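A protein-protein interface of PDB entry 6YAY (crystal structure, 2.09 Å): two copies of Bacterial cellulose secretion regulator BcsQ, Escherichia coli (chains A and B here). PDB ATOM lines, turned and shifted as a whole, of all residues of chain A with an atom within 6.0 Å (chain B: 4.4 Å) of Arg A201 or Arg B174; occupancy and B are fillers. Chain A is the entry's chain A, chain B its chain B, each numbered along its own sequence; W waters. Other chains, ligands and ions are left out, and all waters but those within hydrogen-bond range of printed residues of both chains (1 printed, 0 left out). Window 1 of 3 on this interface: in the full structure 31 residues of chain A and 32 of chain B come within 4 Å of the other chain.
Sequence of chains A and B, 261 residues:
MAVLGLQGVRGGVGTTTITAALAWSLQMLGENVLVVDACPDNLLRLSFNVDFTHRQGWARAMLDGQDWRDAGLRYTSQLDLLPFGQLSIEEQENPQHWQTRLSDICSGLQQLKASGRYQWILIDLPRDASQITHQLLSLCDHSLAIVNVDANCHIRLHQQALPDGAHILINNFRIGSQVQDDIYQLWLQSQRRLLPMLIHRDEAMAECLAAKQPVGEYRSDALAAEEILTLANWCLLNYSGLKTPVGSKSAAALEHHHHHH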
ATOM      1  N   ASN A 171      27.300 -12.483 -37.211  1.00  0.00           N
ATOM      2  CA  ASN A 171      28.124 -12.239 -36.038  1.00  0.00           C
ATOM      3  C   ASN A 171      27.422 -12.810 -34.812  1.00  0.00           C
ATOM      4  O   ASN A 171      26.213 -13.067 -34.830  1.00  0.00           O
ATOM      5  CB  ASN A 171      28.396 -10.738 -35.848  1.00  0.00           C
ATOM      6  CG  ASN A 171      29.350 -10.455 -34.700  1.00  0.00           C
ATOM      7  OD1 ASN A 171      30.332 -11.173 -34.497  1.00  0.00           O
ATOM      8  ND2 ASN A 171      29.053  -9.416 -33.930  1.00  0.00           N
ATOM      9  N   ASN A 172      28.204 -13.037 -33.754  1.00  0.00           N
ATOM     10  CA  ASN A 172      27.681 -13.451 -32.451  1.00  0.00           C
ATOM     11  C   ASN A 172      27.015 -14.821 -32.507  1.00  0.00           C
ATOM     12  O   ASN A 172      26.142 -15.127 -31.693  1.00  0.00           O
ATOM     13  CB  ASN A 172      26.701 -12.414 -31.893  1.00  0.00           C
ATOM     14  CG  ASN A 172      27.250 -11.683 -30.692  1.00  0.00           C
ATOM     15  OD1 ASN A 172      27.877 -12.286 -29.821  1.00  0.00           O
ATOM     16  ND2 ASN A 172      27.019 -10.376 -30.636  1.00  0.00           N
ATOM     17  N   PHE A 173      27.414 -15.656 -33.460  1.00  0.00           N
ATOM     18  CA  PHE A 173      26.796 -16.963 -33.615  1.00  0.00           C
ATOM     19  C   PHE A 173      27.235 -17.904 -32.498  1.00  0.00           C
ATOM     20  O   PHE A 173      28.362 -17.830 -32.000  1.00  0.00           O
ATOM     21  CB  PHE A 173      27.158 -17.560 -34.974  1.00  0.00           C
ATOM     22  CG  PHE A 173      26.531 -18.895 -35.236  1.00  0.00           C
ATOM     23  CD1 PHE A 173      25.218 -18.985 -35.659  1.00  0.00           C
ATOM     24  CD2 PHE A 173      27.254 -20.062 -35.061  1.00  0.00           C
ATOM     25  CE1 PHE A 173      24.636 -20.216 -35.905  1.00  0.00           C
ATOM     26  CE2 PHE A 173      26.678 -21.294 -35.305  1.00  0.00           C
ATOM     27  CZ  PHE A 173      25.366 -21.370 -35.727  1.00  0.00           C
ATOM     28  N   ARG A 174      26.327 -18.798 -32.104  1.00  0.00           N
ATOM     29  CA  ARG A 174      26.628 -19.806 -31.095  1.00  0.00           C
ATOM     30  C   ARG A 174      25.582 -20.909 -31.168  1.00  0.00           C
ATOM     31  O   ARG A 174      24.380 -20.625 -31.171  1.00  0.00           O
ATOM     32  CB  ARG A 174      26.660 -19.197 -29.691  1.00  0.00           C
ATOM     33  CG  ARG A 174      27.279 -20.103 -28.643  1.00  0.00           C
ATOM     34  CD  ARG A 174      27.343 -19.416 -27.292  1.00  0.00           C
ATOM     35  NE  ARG A 174      28.324 -20.043 -26.414  1.00  0.00           N
ATOM     36  CZ  ARG A 174      28.556 -19.668 -25.161  1.00  0.00           C
ATOM     37  NH1 ARG A 174      29.472 -20.298 -24.436  1.00  0.00           N
ATOM     38  NH2 ARG A 174      27.869 -18.664 -24.628  1.00  0.00           N
ATOM     39  N   ILE A 199      31.226 -15.121 -37.659  1.00  0.00           N
ATOM     40  CA  ILE A 199      31.975 -14.792 -36.451  1.00  0.00           C
ATOM     41  C   ILE A 199      31.198 -15.335 -35.258  1.00  0.00           C
ATOM     42  O   ILE A 199      30.076 -14.888 -34.989  1.00  0.00           O
ATOM     43  CB  ILE A 199      32.198 -13.278 -36.318  1.00  0.00           C
ATOM     44  CG1 ILE A 199      32.594 -12.662 -37.665  1.00  0.00           C
ATOM     45  CG2 ILE A 199      33.245 -12.989 -35.248  1.00  0.00           C
ATOM     46  CD1 ILE A 199      33.876 -13.217 -38.253  1.00  0.00           C
ATOM     47  N   HIS A 200      31.784 -16.298 -34.551  1.00  0.00           N
ATOM     48  CA  HIS A 200      31.165 -16.822 -33.341  1.00  0.00           C
ATOM     49  C   HIS A 200      31.152 -15.767 -32.238  1.00  0.00           C
ATOM     50  O   HIS A 200      31.966 -14.840 -32.216  1.00  0.00           O
ATOM     51  CB  HIS A 200      31.912 -18.058 -32.829  1.00  0.00           C
ATOM     52  CG  HIS A 200      31.683 -19.296 -33.639  1.00  0.00           C
ATOM     53  ND1 HIS A 200      32.341 -19.544 -34.825  1.00  0.00           N
ATOM     54  CD2 HIS A 200      30.880 -20.365 -33.423  1.00  0.00           C
ATOM     55  CE1 HIS A 200      31.946 -20.708 -35.309  1.00  0.00           C
ATOM     56  NE2 HIS A 200      31.061 -21.227 -34.477  1.00  0.00           N
ATOM     57  N   ARG A 201      30.215 -15.924 -31.305  1.00  0.00           N
ATOM     58  CA  ARG A 201      30.302 -15.166 -30.066  1.00  0.00           C
ATOM     59  C   ARG A 201      31.607 -15.521 -29.370  1.00  0.00           C
ATOM     60  O   ARG A 201      32.030 -16.678 -29.363  1.00  0.00           O
ATOM     61  CB  ARG A 201      29.114 -15.465 -29.146  1.00  0.00           C
ATOM     62  CG  ARG A 201      29.126 -14.636 -27.859  1.00  0.00           C
ATOM     63  CD  ARG A 201      27.970 -14.954 -26.920  1.00  0.00           C
ATOM     64  NE  ARG A 201      26.701 -14.402 -27.381  1.00  0.00           N
ATOM     65  CZ  ARG A 201      26.327 -13.139 -27.200  1.00  0.00           C
ATOM     66  NH1 ARG A 201      27.130 -12.286 -26.576  1.00  0.00           N
ATOM     67  NH2 ARG A 201      25.149 -12.730 -27.650  1.00  0.00           N
ATOM     68  N   ASP A 202      32.253 -14.516 -28.788  1.00  0.00           N
ATOM     69  CA  ASP A 202      33.579 -14.703 -28.216  1.00  0.00           C
ATOM     70  C   ASP A 202      33.794 -13.617 -27.177  1.00  0.00           C
ATOM     71  O   ASP A 202      33.621 -12.434 -27.479  1.00  0.00           O
ATOM     72  CB  ASP A 202      34.652 -14.633 -29.311  1.00  0.00           C
ATOM     73  CG  ASP A 202      36.010 -15.105 -28.837  1.00  0.00           C
ATOM     74  OD1 ASP A 202      36.360 -14.871 -27.662  1.00  0.00           O
ATOM     75  OD2 ASP A 202      36.732 -15.713 -29.652  1.00  0.00           O
ATOM     76  N   GLU A 203      34.161 -14.019 -25.959  1.00  0.00           N
ATOM     77  CA  GLU A 203      34.402 -13.033 -24.915  1.00  0.00           C
ATOM     78  C   GLU A 203      35.509 -12.058 -25.293  1.00  0.00           C
ATOM     79  O   GLU A 203      35.526 -10.934 -24.783  1.00  0.00           O
ATOM     80  CB  GLU A 203      34.725 -13.730 -23.594  1.00  0.00           C
ATOM     81  CG  GLU A 203      33.522 -14.434 -22.979  1.00  0.00           C
ATOM     82  CD  GLU A 203      32.329 -13.504 -22.821  1.00  0.00           C
ATOM     83  OE1 GLU A 203      32.526 -12.360 -22.359  1.00  0.00           O
ATOM     84  OE2 GLU A 203      31.198 -13.911 -23.168  1.00  0.00           O
ATOM     85  N   MET A 205      35.673 -10.605 -28.120  1.00  0.00           N
ATOM     86  CA  MET A 205      34.932  -9.553 -28.813  1.00  0.00           C
ATOM     87  C   MET A 205      34.220  -8.630 -27.831  1.00  0.00           C
ATOM     88  O   MET A 205      33.976  -7.460 -28.128  1.00  0.00           O
ATOM     89  CB  MET A 205      33.911 -10.157 -29.778  1.00  0.00           C
ATOM     90  CG  MET A 205      34.515 -10.868 -30.975  1.00  0.00           C
ATOM     91  SD  MET A 205      35.080  -9.672 -32.411  1.00  0.00           S
ATOM     92  CE  MET A 205      33.325  -9.102 -33.051  1.00  0.00           C
ATOM     93  N   ALA A 206      33.874  -9.166 -26.660  1.00  0.00           N
ATOM     94  CA  ALA A 206      33.252  -8.341 -25.632  1.00  0.00           C
ATOM     95  C   ALA A 206      34.287  -7.581 -24.814  1.00  0.00           C
ATOM     96  O   ALA A 206      34.007  -6.472 -24.346  1.00  0.00           O
ATOM     97  CB  ALA A 206      32.381  -9.200 -24.713  1.00  0.00           C
ATOM     98  N   LEU A 223      39.222 -17.270 -31.281  1.00  0.00           N
ATOM     99  CA  LEU A 223      38.500 -17.814 -32.427  1.00  0.00           C
ATOM    100  C   LEU A 223      37.940 -16.702 -33.304  1.00  0.00           C
ATOM    101  O   LEU A 223      38.021 -16.772 -34.536  1.00  0.00           O
ATOM    102  CB  LEU A 223      37.378 -18.738 -31.954  1.00  0.00           C
ATOM    103  CG  LEU A 223      36.442 -19.255 -33.048  1.00  0.00           C
ATOM    104  CD1 LEU A 223      37.211 -20.050 -34.088  1.00  0.00           C
ATOM    105  CD2 LEU A 223      35.328 -20.093 -32.449  1.00  0.00           C
ATOM    106  N   ALA A 224      37.376 -15.662 -32.686  1.00  0.00           N
ATOM    107  CA  ALA A 224      36.822 -14.559 -33.464  1.00  0.00           C
ATOM    108  C   ALA A 224      37.912 -13.812 -34.224  1.00  0.00           C
ATOM    109  O   ALA A 224      37.683 -13.349 -35.348  1.00  0.00           O
ATOM    110  CB  ALA A 224      36.054 -13.608 -32.550  1.00  0.00           C
ATOM    111  N   GLU A 227      38.604 -15.761 -37.149  1.00  0.00           N
ATOM    112  CA  GLU A 227      37.504 -15.620 -38.097  1.00  0.00           C
ATOM    113  C   GLU A 227      37.548 -14.275 -38.813  1.00  0.00           C
ATOM    114  O   GLU A 227      37.200 -14.195 -39.996  1.00  0.00           O
ATOM    115  CB  GLU A 227      36.171 -15.818 -37.377  1.00  0.00           C
ATOM    116  CG  GLU A 227      35.931 -17.262 -36.948  1.00  0.00           C
ATOM    117  CD  GLU A 227      34.816 -17.406 -35.930  1.00  0.00           C
ATOM    118  OE1 GLU A 227      34.636 -16.489 -35.101  1.00  0.00           O
ATOM    119  OE2 GLU A 227      34.119 -18.444 -35.958  1.00  0.00           O
ATOM    120  N   ASN B 172      18.995  -9.333 -21.330  1.00  0.00           N
ATOM    121  CA  ASN B 172      19.992 -10.215 -21.931  1.00  0.00           C
ATOM    122  C   ASN B 172      21.166 -10.520 -21.008  1.00  0.00           C
ATOM    123  O   ASN B 172      22.246 -10.878 -21.488  1.00  0.00           O
ATOM    124  CB  ASN B 172      20.529  -9.646 -23.254  1.00  0.00           C
ATOM    125  CG  ASN B 172      19.615  -9.930 -24.429  1.00  0.00           C
ATOM    126  OD1 ASN B 172      19.017 -11.001 -24.519  1.00  0.00           O
ATOM    127  ND2 ASN B 172      19.508  -8.971 -25.341  1.00  0.00           N
ATOM    128  N   PHE B 173      20.998 -10.381 -19.694  1.00  0.00           N
ATOM    129  CA  PHE B 173      22.044 -10.807 -18.774  1.00  0.00           C
ATOM    130  C   PHE B 173      22.328 -12.290 -18.993  1.00  0.00           C
ATOM    131  O   PHE B 173      21.405 -13.103 -19.095  1.00  0.00           O
ATOM    132  CB  PHE B 173      21.624 -10.534 -17.330  1.00  0.00           C
ATOM    133  CG  PHE B 173      22.778 -10.300 -16.396  1.00  0.00           C
ATOM    134  CD1 PHE B 173      23.471  -9.100 -16.417  1.00  0.00           C
ATOM    135  CD2 PHE B 173      23.162 -11.274 -15.490  1.00  0.00           C
ATOM    136  CE1 PHE B 173      24.532  -8.881 -15.557  1.00  0.00           C
ATOM    137  CE2 PHE B 173      24.219 -11.059 -14.629  1.00  0.00           C
ATOM    138  CZ  PHE B 173      24.902  -9.861 -14.660  1.00  0.00           C
ATOM    139  N   ARG B 174      23.615 -12.634 -19.038  1.00  0.00           N
ATOM    140  CA  ARG B 174      24.075 -13.921 -19.537  1.00  0.00           C
ATOM    141  C   ARG B 174      25.116 -14.507 -18.589  1.00  0.00           C
ATOM    142  O   ARG B 174      25.760 -13.788 -17.821  1.00  0.00           O
ATOM    143  CB  ARG B 174      24.666 -13.762 -20.949  1.00  0.00           C
ATOM    144  CG  ARG B 174      24.881 -15.050 -21.726  1.00  0.00           C
ATOM    145  CD  ARG B 174      25.322 -14.757 -23.158  1.00  0.00           C
ATOM    146  NE  ARG B 174      26.475 -13.860 -23.204  1.00  0.00           N
ATOM    147  CZ  ARG B 174      27.736 -14.257 -23.071  1.00  0.00           C
ATOM    148  NH1 ARG B 174      28.014 -15.540 -22.882  1.00  0.00           N
ATOM    149  NH2 ARG B 174      28.722 -13.372 -23.125  1.00  0.00           N
ATOM    150  N   ILE B 175      25.271 -15.837 -18.648  1.00  0.00           N
ATOM    151  CA  ILE B 175      26.360 -16.531 -17.971  1.00  0.00           C
ATOM    152  C   ILE B 175      27.553 -16.555 -18.914  1.00  0.00           C
ATOM    153  O   ILE B 175      27.397 -16.531 -20.139  1.00  0.00           O
ATOM    154  CB  ILE B 175      25.948 -17.964 -17.567  1.00  0.00           C
ATOM    155  CG1 ILE B 175      24.589 -17.967 -16.871  1.00  0.00           C
ATOM    156  CG2 ILE B 175      27.018 -18.623 -16.681  1.00  0.00           C
ATOM    157  CD1 ILE B 175      24.584 -17.321 -15.510  1.00  0.00           C
ATOM    158  N   GLY B 176      28.757 -16.588 -18.343  1.00  0.00           N
ATOM    159  CA  GLY B 176      29.961 -16.833 -19.111  1.00  0.00           C
ATOM    160  C   GLY B 176      30.693 -15.611 -19.613  1.00  0.00           C
ATOM    161  O   GLY B 176      31.474 -15.725 -20.566  1.00  0.00           O
ATOM    162  N   SER B 177      30.485 -14.447 -19.006  1.00  0.00           N
ATOM    163  CA  SER B 177      31.124 -13.214 -19.454  1.00  0.00           C
ATOM    164  C   SER B 177      31.689 -12.482 -18.247  1.00  0.00           C
ATOM    165  O   SER B 177      30.934 -11.907 -17.456  1.00  0.00           O
ATOM    166  CB  SER B 177      30.141 -12.325 -20.217  1.00  0.00           C
ATOM    167  OG  SER B 177      30.767 -11.123 -20.633  1.00  0.00           O
ATOM    168  N   GLN B 180      31.150  -8.565 -18.614  1.00  0.00           N
ATOM    169  CA  GLN B 180      29.787  -8.181 -18.253  1.00  0.00           C
ATOM    170  C   GLN B 180      29.622  -8.099 -16.742  1.00  0.00           C
ATOM    171  O   GLN B 180      28.985  -7.173 -16.227  1.00  0.00           O
ATOM    172  CB  GLN B 180      28.776  -9.168 -18.839  1.00  0.00           C
ATOM    173  CG  GLN B 180      27.355  -8.938 -18.350  1.00  0.00           C
ATOM    174  CD  GLN B 180      26.505 -10.196 -18.381  1.00  0.00           C
ATOM    175  OE1 GLN B 180      25.714 -10.403 -19.300  1.00  0.00           O
ATOM    176  NE2 GLN B 180      26.664 -11.043 -17.370  1.00  0.00           N
HETATM  177  O   HOH W   1      34.181 -11.452 -20.286  1.00  0.00           O
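The side-chain carboxylate of Glu A203 is in salt-bridge range of the guanidinium group of Arg B174 (2.5 Å). OE1 of Glu A203 lies within hydrogen-bond range of OG of Ser B177 (2.8 Å). The side-chain carboxylate (OE2) of Glu A203 sits close to the backbone carbonyl oxygen (O) of Gly B176.
The side-chain amide oxygen of Asn A172 sits close to the guanidinium group of Arg A201 (3.3 Å). N of Arg A201 is in hydrogen-bond range of O of Phe A173 (2.7 Å). O of Arg B174 is in hydrogen-bond range of NE2 of Gln B180, at 2.9 Å. OG of Ser B177 lies within hydrogen-bond range of N of Gln B180, at 3.3 Å.
NH1 of Arg B174 touches NH2 of Arg A174, 3.6 Å away. Arg A201 touches Arg B174.
Printed residues of chain B within 4 Å of Arg A201: Arg B174 (3.8 Å). Printed residues of chain A within 4 Å of Arg B174: Arg A174, Arg A201 and Glu A203. Printed residues of chain A within 4 Å of Ser B177: Glu A203. Printed residues of chain B within 4 Å of Glu A203: Arg B174 (2.5 Å), Gly B176 (3.2 Å) and Ser B177 (2.8 Å). Phe B173 touches none of the printed residues of chain A. The nearest printed residue of chain B that does not touch Glu A203 is Gln B180 (5.5 Å).
Of the 14 printed residues of chain A, 3 touch a printed residue of chain B. Printed residues of chain A that touch a printed residue of chain B: Arg A174, Arg A201 and Glu A203. Among the printed residues, 5 pairs touch across the chains.
Arg B174 touches its own counterpart, Arg A174. Of the 5 pairs that touch across the chains among the printed residues, 1 has its exchanged pair printed and touching as well.
Water W1 lies within hydrogen-bond range of the side-chain carboxylate (OE1) of Glu A203 and the side-chain hydroxyl (OG) of Ser B177.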
